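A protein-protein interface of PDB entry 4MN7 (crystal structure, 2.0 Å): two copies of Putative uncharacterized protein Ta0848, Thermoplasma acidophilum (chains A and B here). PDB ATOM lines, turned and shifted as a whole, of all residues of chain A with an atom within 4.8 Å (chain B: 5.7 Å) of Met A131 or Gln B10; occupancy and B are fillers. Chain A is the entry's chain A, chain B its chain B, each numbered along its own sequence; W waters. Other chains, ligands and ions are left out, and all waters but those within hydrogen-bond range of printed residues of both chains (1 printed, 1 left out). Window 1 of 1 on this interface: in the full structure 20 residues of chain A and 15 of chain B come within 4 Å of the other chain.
The side-chain amide oxygen (OE1) of Gln A10 lies close to the side-chain sulfur (SD) of Met B131 (3.6 Å). The side-chain amide oxygen of Gln A10 sits close to the side-chain amide oxygen of Gln B10, at 2.7 Å. The backbone NH of Ala B14 sits close to the side-chain amide nitrogen of Gln A10, at 3.2 Å. N of Ala A14 sits close to NE2 of Gln B10 (3.0 Å). SD of Met A131 lies close to OE1 of Gln B10, 3.5 Å away.
OG of Ser B9 sits at hydrogen-bond distance from O of Phe B6 (3.0 Å).
Among the printed residues, pairs that only touch across the chains: Gln A10 with Ala B13 (3.7 Å), Ala A13 with Gln B10 (3.6 Å), Ala A13 with Ala B13 (3.8 Å), Ala A14 with Phe B6 (3.95 Å), Ile A127 with Phe B6 (3.7 Å), Leu A130 with Leu B134 (3.8 Å) and Met A131 with Phe B6 (3.9 Å).
Gln B10 touches just these residues of chain A: Gln A10, Ala A13, Ala A14 and Met A131. Of the printed residues of chain A, Ala B13 touches Gln A10 (3.7 Å) and Ala A13 (3.8 Å). Of the printed residues of chain A, Leu B134 touches Leu A130. The nearest residue of chain A that does not touch Gln B10 is Leu A134 (4.4 Å).
Hydrophobic or aromatic side chains of chain A within 4 Å of the printed part of chain B: Ala A13, Ala A14, Ile A127, Leu A130 and Met A131. Printed residues of chain B that touch a printed residue of chain A: Phe B6, Gln B10, Ala B13, Ala B14, Met B131 and Leu B134. Among the printed residues, 12 pairs touch across the chains. Among the printed residues, no Asp or Glu carboxylate lies within 4 Å of a Lys or Arg side-chain nitrogen of the other chain.
Gln B10 touches its own counterpart, Gln A10. Gln A10 touches Ala B13, and with the chains exchanged Ala A13 touches Gln B10. Gln A10 touches Met B131, and with the chains exchanged Met A131 touches Gln B10. Ala A13 touches its own counterpart, Ala B13. Positions printed for both chains: 10, 11, 13, 14, 131 and 134.
Water W1 lies within hydrogen-bond range of the side-chain amide nitrogen of Gln A10 (2.4 Å) and the backbone carbonyl oxygen of Ala B13 (3.4 Å).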
ATOM      1  N   GLN A  10      25.124  22.789  24.459  1.00  0.00           N
ATOM      2  CA  GLN A  10      25.216  21.549  23.648  1.00  0.00           C
ATOM      3  C   GLN A  10      24.158  21.498  22.561  1.00  0.00           C
ATOM      4  O   GLN A  10      24.450  21.223  21.417  1.00  0.00           O
ATOM      5  CB  GLN A  10      25.095  20.314  24.523  1.00  0.00           C
ATOM      6  CG  GLN A  10      26.293  20.094  25.421  1.00  0.00           C
ATOM      7  CD  GLN A  10      27.558  19.781  24.614  1.00  0.00           C
ATOM      8  OE1 GLN A  10      27.603  18.773  23.925  1.00  0.00           O
ATOM      9  NE2 GLN A  10      28.546  20.633  24.694  1.00  0.00           N
ATOM     10  N   MET A  11      22.909  21.746  22.921  1.00  0.00           N
ATOM     11  CA  MET A  11      21.800  21.714  21.948  1.00  0.00           C
ATOM     12  C   MET A  11      22.010  22.758  20.869  1.00  0.00           C
ATOM     13  O   MET A  11      21.798  22.539  19.673  1.00  0.00           O
ATOM     14  CB  MET A  11      20.439  21.967  22.661  1.00  0.00           C
ATOM     15  CG  MET A  11      19.940  20.768  23.425  1.00  0.00           C
ATOM     16  SD  MET A  11      18.275  21.030  24.120  1.00  0.00           S
ATOM     17  CE  MET A  11      18.880  21.572  25.598  1.00  0.00           C
ATOM     18  N   ALA A  13      24.923  24.019  19.886  1.00  0.00           N
ATOM     19  CA  ALA A  13      26.031  23.499  19.041  1.00  0.00           C
ATOM     20  C   ALA A  13      25.508  22.385  18.114  1.00  0.00           C
ATOM     21  O   ALA A  13      25.873  22.336  16.948  1.00  0.00           O
ATOM     22  CB  ALA A  13      27.160  22.938  19.900  1.00  0.00           C
ATOM     23  N   ALA A  14      24.625  21.523  18.617  1.00  0.00           N
ATOM     24  CA  ALA A  14      23.998  20.508  17.736  1.00  0.00           C
ATOM     25  C   ALA A  14      23.172  21.139  16.580  1.00  0.00           C
ATOM     26  O   ALA A  14      23.241  20.715  15.414  1.00  0.00           O
ATOM     27  CB  ALA A  14      23.161  19.537  18.554  1.00  0.00           C
ATOM     28  N   PHE A  30      15.307  22.490  18.783  1.00  0.00           N
ATOM     29  CA  PHE A  30      14.928  21.559  19.769  1.00  0.00           C
ATOM     30  C   PHE A  30      13.761  22.128  20.553  1.00  0.00           C
ATOM     31  O   PHE A  30      13.875  23.206  21.231  1.00  0.00           O
ATOM     32  CB  PHE A  30      16.036  21.234  20.749  1.00  0.00           C
ATOM     33  CG  PHE A  30      17.163  20.351  20.197  1.00  0.00           C
ATOM     34  CD1 PHE A  30      18.061  20.826  19.269  1.00  0.00           C
ATOM     35  CD2 PHE A  30      17.370  19.073  20.684  1.00  0.00           C
ATOM     36  CE1 PHE A  30      19.115  20.022  18.797  1.00  0.00           C
ATOM     37  CE2 PHE A  30      18.441  18.300  20.239  1.00  0.00           C
ATOM     38  CZ  PHE A  30      19.301  18.782  19.281  1.00  0.00           C
ATOM     39  N   ILE A 127      20.995  10.796  16.192  1.00  0.00           N
ATOM     40  CA  ILE A 127      21.372  12.049  16.830  1.00  0.00           C
ATOM     41  C   ILE A 127      20.501  12.395  18.016  1.00  0.00           C
ATOM     42  O   ILE A 127      20.994  12.770  19.112  1.00  0.00           O
ATOM     43  CB  ILE A 127      21.398  13.169  15.804  1.00  0.00           C
ATOM     44  CG1 ILE A 127      22.661  12.919  14.969  1.00  0.00           C
ATOM     45  CG2 ILE A 127      21.501  14.517  16.549  1.00  0.00           C
ATOM     46  CD1 ILE A 127      22.832  13.708  13.749  1.00  0.00           C
ATOM     47  N   ALA A 128      19.191  12.236  17.805  1.00  0.00           N
ATOM     48  CA  ALA A 128      18.234  12.431  18.834  1.00  0.00           C
ATOM     49  C   ALA A 128      18.506  11.567  20.050  1.00  0.00           C
ATOM     50  O   ALA A 128      18.370  12.030  21.192  1.00  0.00           O
ATOM     51  CB  ALA A 128      16.868  12.194  18.321  1.00  0.00           C
ATOM     52  N   ASP A 129      18.969  10.351  19.826  1.00  0.00           N
ATOM     53  CA  ASP A 129      19.223   9.447  20.905  1.00  0.00           C
ATOM     54  C   ASP A 129      20.496   9.860  21.663  1.00  0.00           C
ATOM     55  O   ASP A 129      20.518   9.817  22.897  1.00  0.00           O
ATOM     56  CB  ASP A 129      19.387   8.054  20.350  1.00  0.00           C
ATOM     57  CG  ASP A 129      19.587   7.046  21.411  1.00  0.00           C
ATOM     58  OD1 ASP A 129      18.926   7.138  22.491  1.00  0.00           O
ATOM     59  OD2 ASP A 129      20.417   6.142  21.171  1.00  0.00           O
ATOM     60  N   LEU A 130      21.542  10.276  20.935  1.00  0.00           N
ATOM     61  CA  LEU A 130      22.776  10.713  21.583  1.00  0.00           C
ATOM     62  C   LEU A 130      22.577  11.991  22.420  1.00  0.00           C
ATOM     63  O   LEU A 130      23.199  12.165  23.460  1.00  0.00           O
ATOM     64  CB  LEU A 130      23.902  10.930  20.570  1.00  0.00           C
ATOM     65  CG  LEU A 130      24.298   9.730  19.706  1.00  0.00           C
ATOM     66  CD1 LEU A 130      25.276  10.113  18.609  1.00  0.00           C
ATOM     67  CD2 LEU A 130      24.852   8.667  20.558  1.00  0.00           C
ATOM     68  N   MET A 131      21.676  12.854  21.984  1.00  0.00           N
ATOM     69  CA  MET A 131      21.393  14.127  22.631  1.00  0.00           C
ATOM     70  C   MET A 131      20.377  14.021  23.752  1.00  0.00           C
ATOM     71  O   MET A 131      20.231  14.967  24.545  1.00  0.00           O
ATOM     72  CB  MET A 131      20.866  15.162  21.616  1.00  0.00           C
ATOM     73  CG  MET A 131      21.920  15.549  20.558  1.00  0.00           C
ATOM     74  SD  MET A 131      23.366  16.333  21.352  1.00  0.00           S
ATOM     75  CE  MET A 131      22.646  17.853  21.971  1.00  0.00           C
ATOM     76  N   ALA A 132      19.726  12.877  23.889  1.00  0.00           N
ATOM     77  CA  ALA A 132      18.618  12.812  24.844  1.00  0.00           C
ATOM     78  C   ALA A 132      18.925  13.186  26.298  1.00  0.00           C
ATOM     79  O   ALA A 132      18.140  13.891  26.909  1.00  0.00           O
ATOM     80  CB  ALA A 132      17.942  11.485  24.788  1.00  0.00           C
ATOM     81  N   PRO A 133      20.056  12.747  26.849  1.00  0.00           N
ATOM     82  CA  PRO A 133      20.254  13.146  28.250  1.00  0.00           C
ATOM     83  C   PRO A 133      20.352  14.628  28.399  1.00  0.00           C
ATOM     84  O   PRO A 133      19.929  15.210  29.389  1.00  0.00           O
ATOM     85  CB  PRO A 133      21.611  12.485  28.609  1.00  0.00           C
ATOM     86  CG  PRO A 133      21.572  11.211  27.794  1.00  0.00           C
ATOM     87  CD  PRO A 133      20.927  11.606  26.484  1.00  0.00           C
ATOM     88  N   LEU A 134      20.937  15.261  27.399  1.00  0.00           N
ATOM     89  CA  LEU A 134      21.087  16.656  27.464  1.00  0.00           C
ATOM     90  C   LEU A 134      19.755  17.358  27.343  1.00  0.00           C
ATOM     91  O   LEU A 134      19.496  18.284  28.058  1.00  0.00           O
ATOM     92  CB  LEU A 134      22.038  17.162  26.391  1.00  0.00           C
ATOM     93  CG  LEU A 134      23.489  16.754  26.585  1.00  0.00           C
ATOM     94  CD1 LEU A 134      24.204  16.795  25.241  1.00  0.00           C
ATOM     95  CD2 LEU A 134      24.110  17.705  27.570  1.00  0.00           C
ATOM     96  N   VAL A 135      18.927  16.950  26.408  1.00  0.00           N
ATOM     97  CA  VAL A 135      17.588  17.560  26.216  1.00  0.00           C
ATOM     98  C   VAL A 135      16.749  17.307  27.474  1.00  0.00           C
ATOM     99  O   VAL A 135      15.959  18.119  27.873  1.00  0.00           O
ATOM    100  CB  VAL A 135      16.842  16.878  25.067  1.00  0.00           C
ATOM    101  CG1 VAL A 135      15.362  17.275  25.063  1.00  0.00           C
ATOM    102  CG2 VAL A 135      17.462  17.254  23.770  1.00  0.00           C
ATOM    103  N   GLU B   5      31.990  12.612  13.788  1.00  0.00           N
ATOM    104  CA  GLU B   5      32.320  14.007  13.713  1.00  0.00           C
ATOM    105  C   GLU B   5      31.282  14.820  14.440  1.00  0.00           C
ATOM    106  O   GLU B   5      31.605  15.834  15.049  1.00  0.00           O
ATOM    107  CB  GLU B   5      32.651  14.449  12.249  1.00  0.00           C
ATOM    108  CG  GLU B   5      34.005  13.770  11.749  1.00  0.00           C
ATOM    109  CD  GLU B   5      35.329  13.961  12.627  1.00  0.00           C
ATOM    110  OE1 GLU B   5      35.678  15.080  13.155  1.00  0.00           O
ATOM    111  OE2 GLU B   5      36.093  12.978  12.761  1.00  0.00           O
ATOM    112  N   PHE B   6      30.023  14.401  14.411  1.00  0.00           N
ATOM    113  CA  PHE B   6      29.042  15.027  15.257  1.00  0.00           C
ATOM    114  C   PHE B   6      29.444  14.912  16.738  1.00  0.00           C
ATOM    115  O   PHE B   6      29.466  15.892  17.448  1.00  0.00           O
ATOM    116  CB  PHE B   6      27.716  14.400  15.073  1.00  0.00           C
ATOM    117  CG  PHE B   6      26.670  14.951  16.016  1.00  0.00           C
ATOM    118  CD1 PHE B   6      26.195  16.216  15.845  1.00  0.00           C
ATOM    119  CD2 PHE B   6      26.133  14.177  17.014  1.00  0.00           C
ATOM    120  CE1 PHE B   6      25.225  16.733  16.684  1.00  0.00           C
ATOM    121  CE2 PHE B   6      25.181  14.696  17.867  1.00  0.00           C
ATOM    122  CZ  PHE B   6      24.714  15.987  17.678  1.00  0.00           C
ATOM    123  N   ALA B   7      29.773  13.709  17.211  1.00  0.00           N
ATOM    124  CA  ALA B   7      30.217  13.593  18.586  1.00  0.00           C
ATOM    125  C   ALA B   7      31.422  14.477  18.919  1.00  0.00           C
ATOM    126  O   ALA B   7      31.478  15.062  20.018  1.00  0.00           O
ATOM    127  CB  ALA B   7      30.494  12.166  18.960  1.00  0.00           C
ATOM    128  N   ARG B   8      32.365  14.577  17.980  1.00  0.00           N
ATOM    129  CA  ARG B   8      33.577  15.406  18.174  1.00  0.00           C
ATOM    130  C   ARG B   8      33.198  16.839  18.403  1.00  0.00           C
ATOM    131  O   ARG B   8      33.750  17.437  19.359  1.00  0.00           O
ATOM    132  CB  ARG B   8      34.516  15.316  16.987  1.00  0.00           C
ATOM    133  CG  ARG B   8      35.909  15.929  17.185  1.00  0.00           C
ATOM    134  CD  ARG B   8      36.719  15.641  15.909  1.00  0.00           C
ATOM    135  NE  ARG B   8      37.726  14.812  16.420  1.00  0.00           N
ATOM    136  CZ  ARG B   8      38.092  13.612  16.096  1.00  0.00           C
ATOM    137  NH1 ARG B   8      37.683  12.951  15.036  1.00  0.00           N
ATOM    138  NH2 ARG B   8      39.011  13.134  16.911  1.00  0.00           N
ATOM    139  N   SER B   9      32.244  17.369  17.589  1.00  0.00           N
ATOM    140  CA  SER B   9      31.836  18.760  17.706  1.00  0.00           C
ATOM    141  C   SER B   9      31.136  19.005  19.007  1.00  0.00           C
ATOM    142  O   SER B   9      31.374  20.040  19.594  1.00  0.00           O
ATOM    143  CB  SER B   9      30.978  19.276  16.538  1.00  0.00           C
ATOM    144  OG  SER B   9      29.684  18.828  16.754  1.00  0.00           O
ATOM    145  N   GLN B  10      30.326  18.052  19.503  1.00  0.00           N
ATOM    146  CA  GLN B  10      29.741  18.202  20.841  1.00  0.00           C
ATOM    147  C   GLN B  10      30.797  18.188  21.943  1.00  0.00           C
ATOM    148  O   GLN B  10      30.739  18.960  22.881  1.00  0.00           O
ATOM    149  CB  GLN B  10      28.694  17.127  21.100  1.00  0.00           C
ATOM    150  CG  GLN B  10      27.482  17.248  20.155  1.00  0.00           C
ATOM    151  CD  GLN B  10      26.583  18.377  20.554  1.00  0.00           C
ATOM    152  OE1 GLN B  10      26.164  18.481  21.697  1.00  0.00           O
ATOM    153  NE2 GLN B  10      26.316  19.229  19.642  1.00  0.00           N
ATOM    154  N   MET B  11      31.751  17.275  21.845  1.00  0.00           N
ATOM    155  CA  MET B  11      32.810  17.207  22.850  1.00  0.00           C
ATOM    156  C   MET B  11      33.677  18.508  22.803  1.00  0.00           C
ATOM    157  O   MET B  11      34.007  19.079  23.833  1.00  0.00           O
ATOM    158  CB  MET B  11      33.625  15.940  22.643  1.00  0.00           C
ATOM    159  CG  MET B  11      32.905  14.631  22.972  1.00  0.00           C
ATOM    160  SD  MET B  11      33.595  13.200  22.111  1.00  0.00           S
ATOM    161  CE  MET B  11      35.180  13.128  22.823  1.00  0.00           C
ATOM    162  N   GLN B  12      33.948  19.008  21.601  1.00  0.00           N
ATOM    163  CA  GLN B  12      34.640  20.271  21.441  1.00  0.00           C
ATOM    164  C   GLN B  12      33.878  21.445  22.072  1.00  0.00           C
ATOM    165  O   GLN B  12      34.467  22.231  22.854  1.00  0.00           O
ATOM    166  CB  GLN B  12      34.945  20.509  19.957  1.00  0.00           C
ATOM    167  CG  GLN B  12      35.999  21.551  19.710  1.00  0.00           C
ATOM    168  CD  GLN B  12      37.368  21.250  20.371  1.00  0.00           C
ATOM    169  OE1 GLN B  12      37.926  20.176  20.280  1.00  0.00           O
ATOM    170  NE2 GLN B  12      37.888  22.227  20.994  1.00  0.00           N
ATOM    171  N   ALA B  13      32.579  21.552  21.785  1.00  0.00           N
ATOM    172  CA  ALA B  13      31.719  22.542  22.449  1.00  0.00           C
ATOM    173  C   ALA B  13      31.717  22.390  23.963  1.00  0.00           C
ATOM    174  O   ALA B  13      31.712  23.408  24.689  1.00  0.00           O
ATOM    175  CB  ALA B  13      30.305  22.478  21.947  1.00  0.00           C
ATOM    176  N   ALA B  14      31.706  21.163  24.468  1.00  0.00           N
ATOM    177  CA  ALA B  14      31.716  21.012  25.930  1.00  0.00           C
ATOM    178  C   ALA B  14      33.057  21.526  26.541  1.00  0.00           C
ATOM    179  O   ALA B  14      33.038  22.152  27.590  1.00  0.00           O
ATOM    180  CB  ALA B  14      31.523  19.566  26.300  1.00  0.00           C
ATOM    181  N   CYS B  15      34.195  21.185  25.912  1.00  0.00           N
ATOM    182  CA  CYS B  15      35.523  21.695  26.366  1.00  0.00           C
ATOM    183  C   CYS B  15      35.518  23.218  26.418  1.00  0.00           C
ATOM    184  O   CYS B  15      35.943  23.812  27.399  1.00  0.00           O
ATOM    185  CB  CYS B  15      36.651  21.216  25.435  1.00  0.00           C
ATOM    186  SG  CYS B  15      36.883  19.456  25.507  1.00  0.00           S
ATOM    187  N   MET B 131      27.264  13.510  28.591  1.00  0.00           N
ATOM    188  CA  MET B 131      28.041  13.355  27.372  1.00  0.00           C
ATOM    189  C   MET B 131      28.321  11.925  27.050  1.00  0.00           C
ATOM    190  O   MET B 131      28.868  11.646  25.996  1.00  0.00           O
ATOM    191  CB  MET B 131      29.385  14.057  27.528  1.00  0.00           C
ATOM    192  CG  MET B 131      29.287  15.541  27.767  1.00  0.00           C
ATOM    193  SD  MET B 131      28.463  16.398  26.426  1.00  0.00           S
ATOM    194  CE  MET B 131      29.673  16.276  25.129  1.00  0.00           C
ATOM    195  N   LEU B 134      27.584  10.374  23.555  1.00  0.00           N
ATOM    196  CA  LEU B 134      28.437  10.995  22.538  1.00  0.00           C
ATOM    197  C   LEU B 134      29.844  10.447  22.566  1.00  0.00           C
ATOM    198  O   LEU B 134      30.356  10.001  21.554  1.00  0.00           O
ATOM    199  CB  LEU B 134      28.436  12.515  22.704  1.00  0.00           C
ATOM    200  CG  LEU B 134      27.072  13.127  22.394  1.00  0.00           C
ATOM    201  CD1 LEU B 134      26.796  14.487  23.081  1.00  0.00           C
ATOM    202  CD2 LEU B 134      26.883  13.277  20.896  1.00  0.00           C
HETATM  203  O   HOH W   1      28.614  22.770  25.848  1.00  0.00           O
